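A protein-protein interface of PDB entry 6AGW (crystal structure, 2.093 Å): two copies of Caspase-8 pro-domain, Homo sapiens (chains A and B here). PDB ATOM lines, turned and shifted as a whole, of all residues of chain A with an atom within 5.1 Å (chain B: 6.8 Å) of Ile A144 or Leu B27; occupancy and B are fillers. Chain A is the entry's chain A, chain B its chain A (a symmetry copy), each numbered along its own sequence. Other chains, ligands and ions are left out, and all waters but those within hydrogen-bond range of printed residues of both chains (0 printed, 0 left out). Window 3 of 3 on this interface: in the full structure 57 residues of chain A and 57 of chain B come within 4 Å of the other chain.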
ATOM      1  N   LEU A 140     -14.991 -15.255  -8.595  1.00  0.00           N
ATOM      2  CA  LEU A 140     -14.236 -14.376  -7.701  1.00  0.00           C
ATOM      3  C   LEU A 140     -14.629 -12.906  -7.913  1.00  0.00           C
ATOM      4  O   LEU A 140     -14.713 -12.136  -6.955  1.00  0.00           O
ATOM      5  CB  LEU A 140     -12.726 -14.566  -7.886  1.00  0.00           C
ATOM      6  CG  LEU A 140     -12.104 -15.912  -7.427  1.00  0.00           C
ATOM      7  CD1 LEU A 140     -10.613 -15.870  -7.564  1.00  0.00           C
ATOM      8  CD2 LEU A 140     -12.471 -16.235  -6.003  1.00  0.00           C
ATOM      9  N   ASP A 141     -14.890 -12.521  -9.160  1.00  0.00           N
ATOM     10  CA  ASP A 141     -15.260 -11.125  -9.452  1.00  0.00           C
ATOM     11  C   ASP A 141     -16.632 -10.802  -8.870  1.00  0.00           C
ATOM     12  O   ASP A 141     -16.879  -9.698  -8.394  1.00  0.00           O
ATOM     13  CB  ASP A 141     -15.247 -10.855 -10.964  1.00  0.00           C
ATOM     14  CG  ASP A 141     -13.836 -10.684 -11.513  1.00  0.00           C
ATOM     15  OD1 ASP A 141     -12.948 -10.253 -10.746  1.00  0.00           O
ATOM     16  OD2 ASP A 141     -13.610 -10.982 -12.705  1.00  0.00           O
ATOM     17  N   ILE A 142     -17.509 -11.796  -8.912  1.00  0.00           N
ATOM     18  CA  ILE A 142     -18.812 -11.731  -8.278  1.00  0.00           C
ATOM     19  C   ILE A 142     -18.674 -11.580  -6.774  1.00  0.00           C
ATOM     20  O   ILE A 142     -19.326 -10.709  -6.183  1.00  0.00           O
ATOM     21  CB  ILE A 142     -19.636 -12.985  -8.616  1.00  0.00           C
ATOM     22  CG1 ILE A 142     -19.856 -13.058 -10.131  1.00  0.00           C
ATOM     23  CG2 ILE A 142     -20.955 -12.999  -7.845  1.00  0.00           C
ATOM     24  CD1 ILE A 142     -20.775 -14.153 -10.577  1.00  0.00           C
ATOM     25  N   PHE A 143     -17.828 -12.413  -6.149  1.00  0.00           N
ATOM     26  CA  PHE A 143     -17.590 -12.284  -4.707  1.00  0.00           C
ATOM     27  C   PHE A 143     -17.175 -10.836  -4.388  1.00  0.00           C
ATOM     28  O   PHE A 143     -17.704 -10.204  -3.460  1.00  0.00           O
ATOM     29  CB  PHE A 143     -16.512 -13.284  -4.223  1.00  0.00           C
ATOM     30  CG  PHE A 143     -16.997 -14.727  -4.144  1.00  0.00           C
ATOM     31  CD1 PHE A 143     -18.358 -15.021  -4.074  1.00  0.00           C
ATOM     32  CD2 PHE A 143     -16.092 -15.780  -4.148  1.00  0.00           C
ATOM     33  CE1 PHE A 143     -18.816 -16.349  -4.004  1.00  0.00           C
ATOM     34  CE2 PHE A 143     -16.539 -17.099  -4.076  1.00  0.00           C
ATOM     35  CZ  PHE A 143     -17.906 -17.379  -4.000  1.00  0.00           C
ATOM     36  N   ILE A 144     -16.254 -10.305  -5.186  1.00  0.00           N
ATOM     37  CA  ILE A 144     -15.731  -8.960  -4.967  1.00  0.00           C
ATOM     38  C   ILE A 144     -16.864  -7.944  -5.050  1.00  0.00           C
ATOM     39  O   ILE A 144     -16.924  -7.002  -4.252  1.00  0.00           O
ATOM     40  CB  ILE A 144     -14.618  -8.607  -5.985  1.00  0.00           C
ATOM     41  CG1 ILE A 144     -13.391  -9.493  -5.746  1.00  0.00           C
ATOM     42  CG2 ILE A 144     -14.222  -7.136  -5.884  1.00  0.00           C
ATOM     43  CD1 ILE A 144     -12.244  -9.263  -6.732  1.00  0.00           C
ATOM     44  N   GLU A 145     -17.773  -8.162  -5.996  1.00  0.00           N
ATOM     45  CA  GLU A 145     -18.941  -7.298  -6.148  1.00  0.00           C
ATOM     46  C   GLU A 145     -19.913  -7.484  -4.971  1.00  0.00           C
ATOM     47  O   GLU A 145     -20.384  -6.508  -4.397  1.00  0.00           O
ATOM     48  CB  GLU A 145     -19.633  -7.568  -7.490  1.00  0.00           C
ATOM     49  CG  GLU A 145     -20.836  -6.675  -7.788  1.00  0.00           C
ATOM     50  CD  GLU A 145     -20.535  -5.185  -7.668  1.00  0.00           C
ATOM     51  OE1 GLU A 145     -19.445  -4.742  -8.089  1.00  0.00           O
ATOM     52  OE2 GLU A 145     -21.404  -4.451  -7.153  1.00  0.00           O
ATOM     53  N   MET A 146     -20.193  -8.733  -4.605  1.00  0.00           N
ATOM     54  CA  MET A 146     -21.020  -9.015  -3.434  1.00  0.00           C
ATOM     55  C   MET A 146     -20.476  -8.328  -2.169  1.00  0.00           C
ATOM     56  O   MET A 146     -21.247  -7.865  -1.331  1.00  0.00           O
ATOM     57  CB  MET A 146     -21.128 -10.524  -3.206  1.00  0.00           C
ATOM     58  CG  MET A 146     -21.882 -11.272  -4.302  1.00  0.00           C
ATOM     59  SD  MET A 146     -22.090 -12.989  -3.868  1.00  0.00           S
ATOM     60  CE  MET A 146     -23.278 -12.840  -2.525  1.00  0.00           C
ATOM     61  N   GLU A 147     -19.150  -8.252  -2.050  1.00  0.00           N
ATOM     62  CA  GLU A 147     -18.514  -7.585  -0.913  1.00  0.00           C
ATOM     63  C   GLU A 147     -18.658  -6.064  -0.949  1.00  0.00           C
ATOM     64  O   GLU A 147     -18.712  -5.434   0.100  1.00  0.00           O
ATOM     65  CB  GLU A 147     -17.030  -7.946  -0.835  1.00  0.00           C
ATOM     66  CG  GLU A 147     -16.736  -9.299  -0.212  1.00  0.00           C
ATOM     67  CD  GLU A 147     -15.243  -9.553  -0.071  1.00  0.00           C
ATOM     68  OE1 GLU A 147     -14.455  -8.870  -0.751  1.00  0.00           O
ATOM     69  OE2 GLU A 147     -14.856 -10.418   0.732  1.00  0.00           O
ATOM     70  N   LYS A 148     -18.708  -5.461  -2.136  1.00  0.00           N
ATOM     71  CA  LYS A 148     -19.028  -4.029  -2.208  1.00  0.00           C
ATOM     72  C   LYS A 148     -20.498  -3.757  -1.872  1.00  0.00           C
ATOM     73  O   LYS A 148     -20.838  -2.679  -1.404  1.00  0.00           O
ATOM     74  CB  LYS A 148     -18.726  -3.457  -3.586  1.00  0.00           C
ATOM     75  CG  LYS A 148     -17.333  -3.671  -4.098  1.00  0.00           C
ATOM     76  CD  LYS A 148     -17.445  -4.263  -5.487  1.00  0.00           C
ATOM     77  CE  LYS A 148     -17.112  -3.272  -6.569  1.00  0.00           C
ATOM     78  NZ  LYS A 148     -16.280  -3.938  -7.620  1.00  0.00           N
ATOM     79  N   LEU B  22      -4.411 -15.177  -6.875  1.00  0.00           N
ATOM     80  CA  LEU B  22      -3.454 -14.501  -6.000  1.00  0.00           C
ATOM     81  C   LEU B  22      -3.949 -13.095  -5.667  1.00  0.00           C
ATOM     82  O   LEU B  22      -3.822 -12.625  -4.529  1.00  0.00           O
ATOM     83  CB  LEU B  22      -2.062 -14.454  -6.648  1.00  0.00           C
ATOM     84  CG  LEU B  22      -1.334 -15.803  -6.732  1.00  0.00           C
ATOM     85  CD1 LEU B  22      -0.076 -15.650  -7.596  1.00  0.00           C
ATOM     86  CD2 LEU B  22      -0.994 -16.358  -5.329  1.00  0.00           C
ATOM     87  N   LYS B  23      -4.514 -12.424  -6.667  1.00  0.00           N
ATOM     88  CA  LYS B  23      -5.029 -11.073  -6.462  1.00  0.00           C
ATOM     89  C   LYS B  23      -6.215 -11.102  -5.496  1.00  0.00           C
ATOM     90  O   LYS B  23      -6.300 -10.268  -4.591  1.00  0.00           O
ATOM     91  CB  LYS B  23      -5.440 -10.434  -7.791  1.00  0.00           C
ATOM     92  CG  LYS B  23      -4.239 -10.046  -8.661  1.00  0.00           C
ATOM     93  CD  LYS B  23      -4.643  -9.829 -10.100  1.00  0.00           C
ATOM     94  CE  LYS B  23      -5.494  -8.571 -10.258  1.00  0.00           C
ATOM     95  NZ  LYS B  23      -5.878  -8.380 -11.688  1.00  0.00           N
ATOM     96  N   PHE B  24      -7.106 -12.076  -5.681  1.00  0.00           N
ATOM     97  CA  PHE B  24      -8.271 -12.224  -4.801  1.00  0.00           C
ATOM     98  C   PHE B  24      -7.848 -12.449  -3.345  1.00  0.00           C
ATOM     99  O   PHE B  24      -8.353 -11.800  -2.431  1.00  0.00           O
ATOM    100  CB  PHE B  24      -9.160 -13.384  -5.257  1.00  0.00           C
ATOM    101  CG  PHE B  24     -10.341 -13.623  -4.355  1.00  0.00           C
ATOM    102  CD1 PHE B  24     -10.319 -14.637  -3.414  1.00  0.00           C
ATOM    103  CD2 PHE B  24     -11.478 -12.822  -4.452  1.00  0.00           C
ATOM    104  CE1 PHE B  24     -11.426 -14.874  -2.579  1.00  0.00           C
ATOM    105  CE2 PHE B  24     -12.583 -13.041  -3.624  1.00  0.00           C
ATOM    106  CZ  PHE B  24     -12.555 -14.065  -2.686  1.00  0.00           C
ATOM    107  N   LEU B  25      -6.900 -13.363  -3.139  1.00  0.00           N
ATOM    108  CA  LEU B  25      -6.456 -13.713  -1.786  1.00  0.00           C
ATOM    109  C   LEU B  25      -5.718 -12.561  -1.120  1.00  0.00           C
ATOM    110  O   LEU B  25      -5.524 -12.555   0.096  1.00  0.00           O
ATOM    111  CB  LEU B  25      -5.558 -14.955  -1.821  1.00  0.00           C
ATOM    112  CG  LEU B  25      -6.251 -16.263  -2.230  1.00  0.00           C
ATOM    113  CD1 LEU B  25      -5.211 -17.326  -2.502  1.00  0.00           C
ATOM    114  CD2 LEU B  25      -7.211 -16.731  -1.135  1.00  0.00           C
ATOM    115  N   SER B  26      -5.285 -11.591  -1.922  1.00  0.00           N
ATOM    116  CA  SER B  26      -4.555 -10.443  -1.394  1.00  0.00           C
ATOM    117  C   SER B  26      -5.454  -9.238  -1.110  1.00  0.00           C
ATOM    118  O   SER B  26      -4.958  -8.150  -0.845  1.00  0.00           O
ATOM    119  CB  SER B  26      -3.459 -10.019  -2.374  1.00  0.00           C
ATOM    120  OG  SER B  26      -2.404 -10.953  -2.408  1.00  0.00           O
ATOM    121  N   LEU B  27      -6.766  -9.427  -1.176  1.00  0.00           N
ATOM    122  CA  LEU B  27      -7.693  -8.300  -1.214  1.00  0.00           C
ATOM    123  C   LEU B  27      -7.728  -7.496   0.081  1.00  0.00           C
ATOM    124  O   LEU B  27      -8.037  -6.312   0.057  1.00  0.00           O
ATOM    125  CB  LEU B  27      -9.109  -8.780  -1.546  1.00  0.00           C
ATOM    126  CG  LEU B  27      -9.489  -8.641  -3.020  1.00  0.00           C
ATOM    127  CD1 LEU B  27     -10.666  -9.533  -3.382  1.00  0.00           C
ATOM    128  CD2 LEU B  27      -9.798  -7.192  -3.343  1.00  0.00           C
ATOM    129  N   ASP B  28      -7.418  -8.120   1.212  1.00  0.00           N
ATOM    130  CA  ASP B  28      -7.531  -7.391   2.474  1.00  0.00           C
ATOM    131  C   ASP B  28      -6.307  -6.509   2.702  1.00  0.00           C
ATOM    132  O   ASP B  28      -6.262  -5.736   3.657  1.00  0.00           O
ATOM    133  CB  ASP B  28      -7.738  -8.357   3.642  1.00  0.00           C
ATOM    134  CG  ASP B  28      -9.015  -9.187   3.486  1.00  0.00           C
ATOM    135  OD1 ASP B  28     -10.075  -8.580   3.227  1.00  0.00           O
ATOM    136  OD2 ASP B  28      -8.964 -10.438   3.610  1.00  0.00           O
ATOM    137  N   TYR B  29      -5.331  -6.613   1.805  1.00  0.00           N
ATOM    138  CA  TYR B  29      -4.066  -5.888   1.915  1.00  0.00           C
ATOM    139  C   TYR B  29      -3.851  -4.984   0.714  1.00  0.00           C
ATOM    140  O   TYR B  29      -3.496  -3.820   0.857  1.00  0.00           O
ATOM    141  CB  TYR B  29      -2.884  -6.858   2.034  1.00  0.00           C
ATOM    142  CG  TYR B  29      -2.937  -7.704   3.275  1.00  0.00           C
ATOM    143  CD1 TYR B  29      -3.486  -8.981   3.237  1.00  0.00           C
ATOM    144  CD2 TYR B  29      -2.454  -7.223   4.488  1.00  0.00           C
ATOM    145  CE1 TYR B  29      -3.555  -9.757   4.368  1.00  0.00           C
ATOM    146  CE2 TYR B  29      -2.512  -7.993   5.630  1.00  0.00           C
ATOM    147  CZ  TYR B  29      -3.068  -9.259   5.561  1.00  0.00           C
ATOM    148  OH  TYR B  29      -3.138 -10.030   6.680  1.00  0.00           O
ATOM    149  N   ILE B  30      -4.045  -5.558  -0.469  1.00  0.00           N
ATOM    150  CA  ILE B  30      -3.927  -4.851  -1.738  1.00  0.00           C
ATOM    151  C   ILE B  30      -5.333  -4.600  -2.284  1.00  0.00           C
ATOM    152  O   ILE B  30      -5.898  -5.450  -2.977  1.00  0.00           O
ATOM    153  CB  ILE B  30      -3.081  -5.663  -2.734  1.00  0.00           C
ATOM    154  CG1 ILE B  30      -1.706  -5.945  -2.132  1.00  0.00           C
ATOM    155  CG2 ILE B  30      -2.944  -4.943  -4.060  1.00  0.00           C
ATOM    156  CD1 ILE B  30      -0.678  -6.386  -3.150  1.00  0.00           C
ATOM    157  N   PRO B  31      -5.905  -3.424  -1.950  1.00  0.00           N
ATOM    158  CA  PRO B  31      -7.323  -3.065  -2.083  1.00  0.00           C
ATOM    159  C   PRO B  31      -7.908  -3.285  -3.469  1.00  0.00           C
ATOM    160  O   PRO B  31      -7.217  -3.089  -4.467  1.00  0.00           O
ATOM    161  CB  PRO B  31      -7.336  -1.572  -1.735  1.00  0.00           C
ATOM    162  CG  PRO B  31      -6.186  -1.410  -0.832  1.00  0.00           C
ATOM    163  CD  PRO B  31      -5.127  -2.310  -1.386  1.00  0.00           C
ATOM    164  N   GLN B  32      -9.173  -3.690  -3.511  1.00  0.00           N
ATOM    165  CA  GLN B  32      -9.877  -3.863  -4.768  1.00  0.00           C
ATOM    166  C   GLN B  32      -9.702  -2.642  -5.650  1.00  0.00           C
ATOM    167  O   GLN B  32      -9.346  -2.747  -6.828  1.00  0.00           O
ATOM    168  CB  GLN B  32     -11.359  -4.091  -4.520  1.00  0.00           C
ATOM    169  CG  GLN B  32     -12.129  -4.180  -5.802  1.00  0.00           C
ATOM    170  CD  GLN B  32     -13.509  -3.572  -5.706  1.00  0.00           C
ATOM    171  OE1 GLN B  32     -14.069  -3.400  -4.617  1.00  0.00           O
ATOM    172  NE2 GLN B  32     -14.047  -3.191  -6.856  1.00  0.00           N
ATOM    173  N   ARG B  33      -9.964  -1.489  -5.041  1.00  0.00           N
ATOM    174  CA  ARG B  33      -9.930  -0.193  -5.695  1.00  0.00           C
ATOM    175  C   ARG B  33      -8.620   0.114  -6.405  1.00  0.00           C
ATOM    176  O   ARG B  33      -7.630   0.456  -5.760  1.00  0.00           O
ATOM    177  CB  ARG B  33     -10.187   0.918  -4.675  1.00  0.00           C
ATOM    178  CG  ARG B  33     -10.514   2.264  -5.307  1.00  0.00           C
ATOM    179  CD  ARG B  33      -9.624   3.379  -4.762  1.00  0.00           C
ATOM    180  NE  ARG B  33      -9.213   3.135  -3.383  1.00  0.00           N
ATOM    181  CZ  ARG B  33      -8.224   3.785  -2.782  1.00  0.00           C
ATOM    182  NH1 ARG B  33      -7.563   4.734  -3.433  1.00  0.00           N
ATOM    183  NH2 ARG B  33      -7.906   3.495  -1.528  1.00  0.00           N
ATOM    184  N   LYS B  34      -8.611   0.002  -7.728  1.00  0.00           N
ATOM    185  CA  LYS B  34      -7.551   0.612  -8.529  1.00  0.00           C
ATOM    186  C   LYS B  34      -8.039   1.001  -9.920  1.00  0.00           C
ATOM    187  O   LYS B  34      -9.042   0.487 -10.407  1.00  0.00           O
ATOM    188  CB  LYS B  34      -6.341  -0.313  -8.694  1.00  0.00           C
ATOM    189  CG  LYS B  34      -6.211  -1.443  -7.717  1.00  0.00           C
ATOM    190  CD  LYS B  34      -5.112  -2.401  -8.139  1.00  0.00           C
ATOM    191  CE  LYS B  34      -5.253  -3.663  -7.353  1.00  0.00           C
ATOM    192  NZ  LYS B  34      -5.248  -3.291  -5.905  1.00  0.00           N
ATOM    193  N   PHE B  61       4.315 -13.997   3.587  1.00  0.00           N
ATOM    194  CA  PHE B  61       3.088 -13.788   2.805  1.00  0.00           C
ATOM    195  C   PHE B  61       3.114 -14.434   1.413  1.00  0.00           C
ATOM    196  O   PHE B  61       2.115 -15.002   0.974  1.00  0.00           O
ATOM    197  CB  PHE B  61       2.767 -12.302   2.655  1.00  0.00           C
ATOM    198  CG  PHE B  61       1.343 -12.044   2.301  1.00  0.00           C
ATOM    199  CD1 PHE B  61       0.358 -12.116   3.271  1.00  0.00           C
ATOM    200  CD2 PHE B  61       0.972 -11.759   0.993  1.00  0.00           C
ATOM    201  CE1 PHE B  61      -0.971 -11.893   2.947  1.00  0.00           C
ATOM    202  CE2 PHE B  61      -0.360 -11.528   0.667  1.00  0.00           C
ATOM    203  CZ  PHE B  61      -1.329 -11.608   1.637  1.00  0.00           C
ATOM    204  N   ARG B 102     -11.345 -15.681   3.373  1.00  0.00           N
ATOM    205  CA  ARG B 102     -10.852 -15.484   2.010  1.00  0.00           C
ATOM    206  C   ARG B 102     -10.516 -16.828   1.354  1.00  0.00           C
ATOM    207  O   ARG B 102     -10.875 -17.095   0.207  1.00  0.00           O
ATOM    208  CB  ARG B 102      -9.629 -14.557   2.034  1.00  0.00           C
ATOM    209  CG  ARG B 102      -9.196 -13.995   0.697  1.00  0.00           C
ATOM    210  CD  ARG B 102     -10.250 -13.091   0.104  1.00  0.00           C
ATOM    211  NE  ARG B 102     -10.460 -11.860   0.865  1.00  0.00           N
ATOM    212  CZ  ARG B 102     -11.406 -10.977   0.569  1.00  0.00           C
ATOM    213  NH1 ARG B 102     -12.203 -11.199  -0.471  1.00  0.00           N
ATOM    214  NH2 ARG B 102     -11.561  -9.883   1.301  1.00  0.00           N
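The side-chain carboxylate (OE1) of Glu A145 lies within salt-bridge range of the side-chain amino group (NZ) of Lys A148 (3.3 Å).
NH2 of Arg B102 is in salt-bridge range of OD1 of Asp B28 (2.8 Å).
Of the 15 printed residues of chain B, 4 touch a printed residue of chain A.
Hydrophobic or aromatic side chains of chain B that line the printed part of chain A: Phe B24 and Leu B27.
Hydrophobic or aromatic side chains of chain A within 4 Å of the printed part of chain B: Leu A140, Phe A143 and Ile A144.
No position is printed for both chains.
Of the 6 pairs that touch across the chains among the printed residues, none has its exchanged pair printed and touching as well.
Of chain B, only Leu B27 and Gln B32 come within 4 Å of Ile A144.
Leu B27 touches just one residue of chain A: Ile A144 (3.6 Å).
Printed residues of chain B within 4 Å of Phe A143: Phe B24.
Of the printed residues of chain A, Phe B24 touches Leu A140 and Phe A143.
Asp A141 touches none of the printed residues of chain B.
Pro B31 touches none of the printed residues of chain A.
The nearest residue of chain B that does not touch Ile A144 is Phe B24 (4.1 Å).
The nearest printed residue of chain A that does not touch Gln B32 is Glu A145 (5.8 Å).
OE2 of Glu A147 lies within salt-bridge range of NH1 of Arg B102.
NZ of Lys A148 sits close to NE2 of Gln B32 (2.5 Å).
CD1 of Leu A140 touches CB of Phe B24 (3.7 Å).
Phe A143 touches Phe B24 (CB to CE2, 3.98 Å).
CD1 of Leu B27 touches CG1 of Ile A144 (3.6 Å).
CG2 of Ile A144 touches CG of Gln B32, at 3.6 Å.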
